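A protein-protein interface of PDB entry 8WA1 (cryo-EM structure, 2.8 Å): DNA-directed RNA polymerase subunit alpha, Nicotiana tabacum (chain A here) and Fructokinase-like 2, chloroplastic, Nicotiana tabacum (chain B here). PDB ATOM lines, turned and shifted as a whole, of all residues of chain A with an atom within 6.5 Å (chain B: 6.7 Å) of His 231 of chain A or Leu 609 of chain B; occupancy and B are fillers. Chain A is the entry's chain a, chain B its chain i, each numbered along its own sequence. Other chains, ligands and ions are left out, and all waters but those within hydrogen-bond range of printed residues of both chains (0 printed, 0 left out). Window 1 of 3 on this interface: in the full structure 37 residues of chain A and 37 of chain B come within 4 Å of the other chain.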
ATOM      1  N   ILE A 227      -9.857   2.516  20.124  1.00  0.00           N
ATOM      2  CA  ILE A 227     -10.691   1.597  20.901  1.00  0.00           C
ATOM      3  C   ILE A 227     -11.721   0.851  20.048  1.00  0.00           C
ATOM      4  O   ILE A 227     -11.853  -0.371  20.210  1.00  0.00           O
ATOM      5  CB  ILE A 227     -11.378   2.340  22.060  1.00  0.00           C
ATOM      6  CG1 ILE A 227     -10.507   2.288  23.314  1.00  0.00           C
ATOM      7  CG2 ILE A 227     -12.756   1.762  22.353  1.00  0.00           C
ATOM      8  CD1 ILE A 227     -10.231   0.885  23.805  1.00  0.00           C
ATOM      9  N   PRO A 228     -12.469   1.508  19.143  1.00  0.00           N
ATOM     10  CA  PRO A 228     -13.582   0.798  18.479  1.00  0.00           C
ATOM     11  C   PRO A 228     -13.183  -0.479  17.757  1.00  0.00           C
ATOM     12  O   PRO A 228     -14.031  -1.359  17.565  1.00  0.00           O
ATOM     13  CB  PRO A 228     -14.126   1.850  17.504  1.00  0.00           C
ATOM     14  CG  PRO A 228     -13.800   3.136  18.146  1.00  0.00           C
ATOM     15  CD  PRO A 228     -12.453   2.932  18.758  1.00  0.00           C
ATOM     16  N   PHE A 229     -11.921  -0.611  17.344  1.00  0.00           N
ATOM     17  CA  PHE A 229     -11.491  -1.846  16.700  1.00  0.00           C
ATOM     18  C   PHE A 229     -11.524  -3.037  17.650  1.00  0.00           C
ATOM     19  O   PHE A 229     -11.511  -4.183  17.189  1.00  0.00           O
ATOM     20  CB  PHE A 229     -10.086  -1.681  16.117  1.00  0.00           C
ATOM     21  CG  PHE A 229     -10.057  -0.936  14.815  1.00  0.00           C
ATOM     22  CD1 PHE A 229     -10.416  -1.566  13.636  1.00  0.00           C
ATOM     23  CD2 PHE A 229      -9.668   0.393  14.768  1.00  0.00           C
ATOM     24  CE1 PHE A 229     -10.393  -0.886  12.434  1.00  0.00           C
ATOM     25  CE2 PHE A 229      -9.641   1.078  13.569  1.00  0.00           C
ATOM     26  CZ  PHE A 229     -10.004   0.438  12.401  1.00  0.00           C
ATOM     27  N   LEU A 230     -11.568  -2.796  18.960  1.00  0.00           N
ATOM     28  CA  LEU A 230     -11.629  -3.864  19.949  1.00  0.00           C
ATOM     29  C   LEU A 230     -13.053  -4.185  20.390  1.00  0.00           C
ATOM     30  O   LEU A 230     -13.238  -5.017  21.285  1.00  0.00           O
ATOM     31  CB  LEU A 230     -10.772  -3.503  21.165  1.00  0.00           C
ATOM     32  CG  LEU A 230      -9.283  -3.315  20.870  1.00  0.00           C
ATOM     33  CD1 LEU A 230      -8.509  -3.021  22.142  1.00  0.00           C
ATOM     34  CD2 LEU A 230      -8.720  -4.538  20.167  1.00  0.00           C
ATOM     35  N   HIS A 231     -14.055  -3.550  19.792  1.00  0.00           N
ATOM     36  CA  HIS A 231     -15.445  -3.875  20.060  1.00  0.00           C
ATOM     37  C   HIS A 231     -15.888  -5.054  19.197  1.00  0.00           C
ATOM     38  O   HIS A 231     -15.170  -5.508  18.304  1.00  0.00           O
ATOM     39  CB  HIS A 231     -16.343  -2.662  19.804  1.00  0.00           C
ATOM     40  CG  HIS A 231     -16.396  -1.694  20.945  1.00  0.00           C
ATOM     41  ND1 HIS A 231     -16.398  -0.328  20.763  1.00  0.00           N
ATOM     42  CD2 HIS A 231     -16.465  -1.895  22.282  1.00  0.00           C
ATOM     43  CE1 HIS A 231     -16.457   0.271  21.938  1.00  0.00           C
ATOM     44  NE2 HIS A 231     -16.500  -0.657  22.877  1.00  0.00           N
ATOM     45  N   MET A 232     -17.090  -5.552  19.474  1.00  0.00           N
ATOM     46  CA  MET A 232     -17.634  -6.642  18.682  1.00  0.00           C
ATOM     47  C   MET A 232     -18.048  -6.134  17.302  1.00  0.00           C
ATOM     48  O   MET A 232     -18.410  -4.968  17.119  1.00  0.00           O
ATOM     49  CB  MET A 232     -18.824  -7.287  19.393  1.00  0.00           C
ATOM     50  CG  MET A 232     -19.258  -8.621  18.800  1.00  0.00           C
ATOM     51  SD  MET A 232     -20.690  -9.341  19.625  1.00  0.00           S
ATOM     52  CE  MET A 232     -21.943  -8.114  19.264  1.00  0.00           C
ATOM     53  N   GLU A 233     -17.988  -7.031  16.323  1.00  0.00           N
ATOM     54  CA  GLU A 233     -18.299  -6.663  14.950  1.00  0.00           C
ATOM     55  C   GLU A 233     -19.791  -6.394  14.790  1.00  0.00           C
ATOM     56  O   GLU A 233     -20.637  -7.091  15.355  1.00  0.00           O
ATOM     57  CB  GLU A 233     -17.857  -7.768  13.992  1.00  0.00           C
ATOM     58  CG  GLU A 233     -18.044  -7.438  12.522  1.00  0.00           C
ATOM     59  CD  GLU A 233     -17.552  -8.546  11.611  1.00  0.00           C
ATOM     60  OE1 GLU A 233     -17.751  -8.438  10.382  1.00  0.00           O
ATOM     61  OE2 GLU A 233     -16.967  -9.522  12.123  1.00  0.00           O
ATOM     62  N   SER B 336     -12.126 -13.111  24.243  1.00  0.00           N
ATOM     63  CA  SER B 336     -11.807 -11.912  23.478  1.00  0.00           C
ATOM     64  C   SER B 336     -10.303 -11.709  23.361  1.00  0.00           C
ATOM     65  O   SER B 336      -9.831 -11.101  22.393  1.00  0.00           O
ATOM     66  CB  SER B 336     -12.461 -10.690  24.121  1.00  0.00           C
ATOM     67  OG  SER B 336     -12.124  -9.504  23.423  1.00  0.00           O
ATOM     68  N   THR B 561     -19.795   2.608  35.029  1.00  0.00           N
ATOM     69  CA  THR B 561     -18.462   2.002  35.064  1.00  0.00           C
ATOM     70  C   THR B 561     -17.676   2.315  36.340  1.00  0.00           C
ATOM     71  O   THR B 561     -16.528   1.900  36.478  1.00  0.00           O
ATOM     72  CB  THR B 561     -17.641   2.423  33.831  1.00  0.00           C
ATOM     73  OG1 THR B 561     -18.523   2.935  32.826  1.00  0.00           O
ATOM     74  CG2 THR B 561     -16.896   1.241  33.254  1.00  0.00           C
ATOM     75  N   VAL B 604      -7.227  -2.024  31.629  1.00  0.00           N
ATOM     76  CA  VAL B 604      -7.495  -0.674  31.139  1.00  0.00           C
ATOM     77  C   VAL B 604      -8.327  -0.727  29.863  1.00  0.00           C
ATOM     78  O   VAL B 604      -9.275   0.051  29.687  1.00  0.00           O
ATOM     79  CB  VAL B 604      -6.176   0.093  30.928  1.00  0.00           C
ATOM     80  CG1 VAL B 604      -6.442   1.441  30.278  1.00  0.00           C
ATOM     81  CG2 VAL B 604      -5.456   0.278  32.252  1.00  0.00           C
ATOM     82  N   VAL B 605      -7.996  -1.653  28.960  1.00  0.00           N
ATOM     83  CA  VAL B 605      -8.736  -1.770  27.706  1.00  0.00           C
ATOM     84  C   VAL B 605     -10.189  -2.143  27.973  1.00  0.00           C
ATOM     85  O   VAL B 605     -11.109  -1.577  27.372  1.00  0.00           O
ATOM     86  CB  VAL B 605      -8.049  -2.786  26.776  1.00  0.00           C
ATOM     87  CG1 VAL B 605      -9.010  -3.257  25.699  1.00  0.00           C
ATOM     88  CG2 VAL B 605      -6.809  -2.170  26.150  1.00  0.00           C
ATOM     89  N   ASP B 606     -10.421  -3.092  28.882  1.00  0.00           N
ATOM     90  CA  ASP B 606     -11.786  -3.509  29.182  1.00  0.00           C
ATOM     91  C   ASP B 606     -12.569  -2.394  29.862  1.00  0.00           C
ATOM     92  O   ASP B 606     -13.772  -2.233  29.620  1.00  0.00           O
ATOM     93  CB  ASP B 606     -11.773  -4.768  30.049  1.00  0.00           C
ATOM     94  CG  ASP B 606     -11.286  -5.987  29.293  1.00  0.00           C
ATOM     95  OD1 ASP B 606     -10.850  -5.833  28.132  1.00  0.00           O
ATOM     96  OD2 ASP B 606     -11.343  -7.100  29.855  1.00  0.00           O
ATOM     97  N   GLN B 607     -11.905  -1.604  30.709  1.00  0.00           N
ATOM     98  CA  GLN B 607     -12.586  -0.474  31.330  1.00  0.00           C
ATOM     99  C   GLN B 607     -12.981   0.566  30.288  1.00  0.00           C
ATOM    100  O   GLN B 607     -14.102   1.091  30.320  1.00  0.00           O
ATOM    101  CB  GLN B 607     -11.699   0.147  32.407  1.00  0.00           C
ATOM    102  CG  GLN B 607     -12.454   0.995  33.417  1.00  0.00           C
ATOM    103  CD  GLN B 607     -13.291   0.166  34.371  1.00  0.00           C
ATOM    104  OE1 GLN B 607     -14.256   0.658  34.956  1.00  0.00           O
ATOM    105  NE2 GLN B 607     -12.920  -1.097  34.541  1.00  0.00           N
ATOM    106  N   TRP B 608     -12.078   0.869  29.351  1.00  0.00           N
ATOM    107  CA  TRP B 608     -12.416   1.785  28.264  1.00  0.00           C
ATOM    108  C   TRP B 608     -13.572   1.244  27.430  1.00  0.00           C
ATOM    109  O   TRP B 608     -14.484   1.989  27.050  1.00  0.00           O
ATOM    110  CB  TRP B 608     -11.192   2.029  27.379  1.00  0.00           C
ATOM    111  CG  TRP B 608     -10.212   3.028  27.918  1.00  0.00           C
ATOM    112  CD1 TRP B 608      -9.393   2.875  28.996  1.00  0.00           C
ATOM    113  CD2 TRP B 608      -9.930   4.327  27.383  1.00  0.00           C
ATOM    114  NE1 TRP B 608      -8.626   4.000  29.174  1.00  0.00           N
ATOM    115  CE2 TRP B 608      -8.936   4.907  28.197  1.00  0.00           C
ATOM    116  CE3 TRP B 608     -10.425   5.058  26.300  1.00  0.00           C
ATOM    117  CZ2 TRP B 608      -8.428   6.181  27.960  1.00  0.00           C
ATOM    118  CZ3 TRP B 608      -9.920   6.323  26.069  1.00  0.00           C
ATOM    119  CH2 TRP B 608      -8.932   6.873  26.895  1.00  0.00           C
ATOM    120  N   LEU B 609     -13.549  -0.058  27.135  1.00  0.00           N
ATOM    121  CA  LEU B 609     -14.602  -0.652  26.320  1.00  0.00           C
ATOM    122  C   LEU B 609     -15.950  -0.611  27.023  1.00  0.00           C
ATOM    123  O   LEU B 609     -16.974  -0.371  26.376  1.00  0.00           O
ATOM    124  CB  LEU B 609     -14.242  -2.093  25.955  1.00  0.00           C
ATOM    125  CG  LEU B 609     -13.068  -2.296  24.996  1.00  0.00           C
ATOM    126  CD1 LEU B 609     -12.822  -3.777  24.763  1.00  0.00           C
ATOM    127  CD2 LEU B 609     -13.312  -1.577  23.682  1.00  0.00           C
ATOM    128  N   GLN B 610     -15.977  -0.835  28.339  1.00  0.00           N
ATOM    129  CA  GLN B 610     -17.246  -0.761  29.054  1.00  0.00           C
ATOM    130  C   GLN B 610     -17.724   0.678  29.192  1.00  0.00           C
ATOM    131  O   GLN B 610     -18.933   0.934  29.171  1.00  0.00           O
ATOM    132  CB  GLN B 610     -17.129  -1.414  30.430  1.00  0.00           C
ATOM    133  CG  GLN B 610     -18.468  -1.577  31.131  1.00  0.00           C
ATOM    134  CD  GLN B 610     -18.365  -2.322  32.444  1.00  0.00           C
ATOM    135  OE1 GLN B 610     -17.314  -2.339  33.082  1.00  0.00           O
ATOM    136  NE2 GLN B 610     -19.461  -2.950  32.853  1.00  0.00           N
ATOM    137  N   ALA B 611     -16.797   1.629  29.330  1.00  0.00           N
ATOM    138  CA  ALA B 611     -17.193   3.031  29.402  1.00  0.00           C
ATOM    139  C   ALA B 611     -17.763   3.512  28.074  1.00  0.00           C
ATOM    140  O   ALA B 611     -18.685   4.335  28.047  1.00  0.00           O
ATOM    141  CB  ALA B 611     -16.003   3.894  29.821  1.00  0.00           C
ATOM    142  N   ARG B 612     -17.222   3.014  26.960  1.00  0.00           N
ATOM    143  CA  ARG B 612     -17.720   3.431  25.652  1.00  0.00           C
ATOM    144  C   ARG B 612     -19.002   2.696  25.277  1.00  0.00           C
ATOM    145  O   ARG B 612     -19.900   3.281  24.662  1.00  0.00           O
ATOM    146  CB  ARG B 612     -16.644   3.220  24.589  1.00  0.00           C
ATOM    147  CG  ARG B 612     -15.518   4.239  24.657  1.00  0.00           C
ATOM    148  CD  ARG B 612     -16.040   5.645  24.404  1.00  0.00           C
ATOM    149  NE  ARG B 612     -15.024   6.660  24.659  1.00  0.00           N
ATOM    150  CZ  ARG B 612     -14.895   7.315  25.809  1.00  0.00           C
ATOM    151  NH1 ARG B 612     -13.938   8.220  25.955  1.00  0.00           N
ATOM    152  NH2 ARG B 612     -15.725   7.064  26.813  1.00  0.00           N
ATOM    153  N   ARG B 613     -19.108   1.412  25.633  1.00  0.00           N
ATOM    154  CA  ARG B 613     -20.302   0.644  25.298  1.00  0.00           C
ATOM    155  C   ARG B 613     -21.508   1.130  26.092  1.00  0.00           C
ATOM    156  O   ARG B 613     -22.586   1.356  25.531  1.00  0.00           O
ATOM    157  CB  ARG B 613     -20.055  -0.843  25.553  1.00  0.00           C
ATOM    158  CG  ARG B 613     -21.246  -1.732  25.249  1.00  0.00           C
ATOM    159  CD  ARG B 613     -20.999  -3.153  25.719  1.00  0.00           C
ATOM    160  NE  ARG B 613     -20.786  -3.217  27.163  1.00  0.00           N
ATOM    161  CZ  ARG B 613     -20.534  -4.337  27.830  1.00  0.00           C
ATOM    162  NH1 ARG B 613     -20.353  -4.302  29.143  1.00  0.00           N
ATOM    163  NH2 ARG B 613     -20.464  -5.494  27.186  1.00  0.00           N
ATOM    164  N   LEU B 614     -21.345   1.294  27.401  1.00  0.00           N
ATOM    165  CA  LEU B 614     -22.386   1.823  28.270  1.00  0.00           C
ATOM    166  C   LEU B 614     -22.056   3.276  28.576  1.00  0.00           C
ATOM    167  O   LEU B 614     -21.102   3.557  29.308  1.00  0.00           O
ATOM    168  CB  LEU B 614     -22.489   1.009  29.560  1.00  0.00           C
ATOM    169  CG  LEU B 614     -22.747  -0.491  29.403  1.00  0.00           C
ATOM    170  CD1 LEU B 614     -22.777  -1.174  30.760  1.00  0.00           C
ATOM    171  CD2 LEU B 614     -24.041  -0.740  28.647  1.00  0.00           C
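Of the 7 printed residues of chain A, 3 touch a printed residue of chain B. Hydrophobic or aromatic side chains of chain A that line the printed part of chain B: Ile 227, Leu 230 and His 231. Among the printed residues, 6 pairs touch across the chains.
Ile 227 of chain A touches Trp 608 of chain B (CD1 to CB, 3.9 Å). CD2 of Leu 609 of chain B touches CG2 of Ile 227 of chain A, 3.6 Å away. CG1 of Val 605 of chain B touches CD1 of Leu 230 of chain A, at 3.6 Å. Leu 230 of chain A touches Leu 609 of chain B. NE2 of His 231 of chain A touches CD2 of Leu 609 of chain B, at 3.4 Å. His 231 of chain A touches Arg 612 of chain B (CE1 to CB, 3.97 Å).
His 231 of chain A touches just these residues of chain B: Leu 609 and Arg 612. Leu 609 of chain B touches just these residues of chain A: Ile 227, Leu 230 and His 231. Of the printed residues of chain A, Arg 612 of chain B touches His 231. Of the printed residues of chain A, Trp 608 of chain B touches Ile 227. Printed residues of chain A within 4 Å of Val 605 of chain B: Leu 230. Of the printed residues of chain B, Leu 230 of chain A touches Val 605 (3.6 Å) and Leu 609 (3.7 Å). Leu 614 of chain B touches none of the printed residues of chain A. Glu 233 of chain A touches none of the printed residues of chain B.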
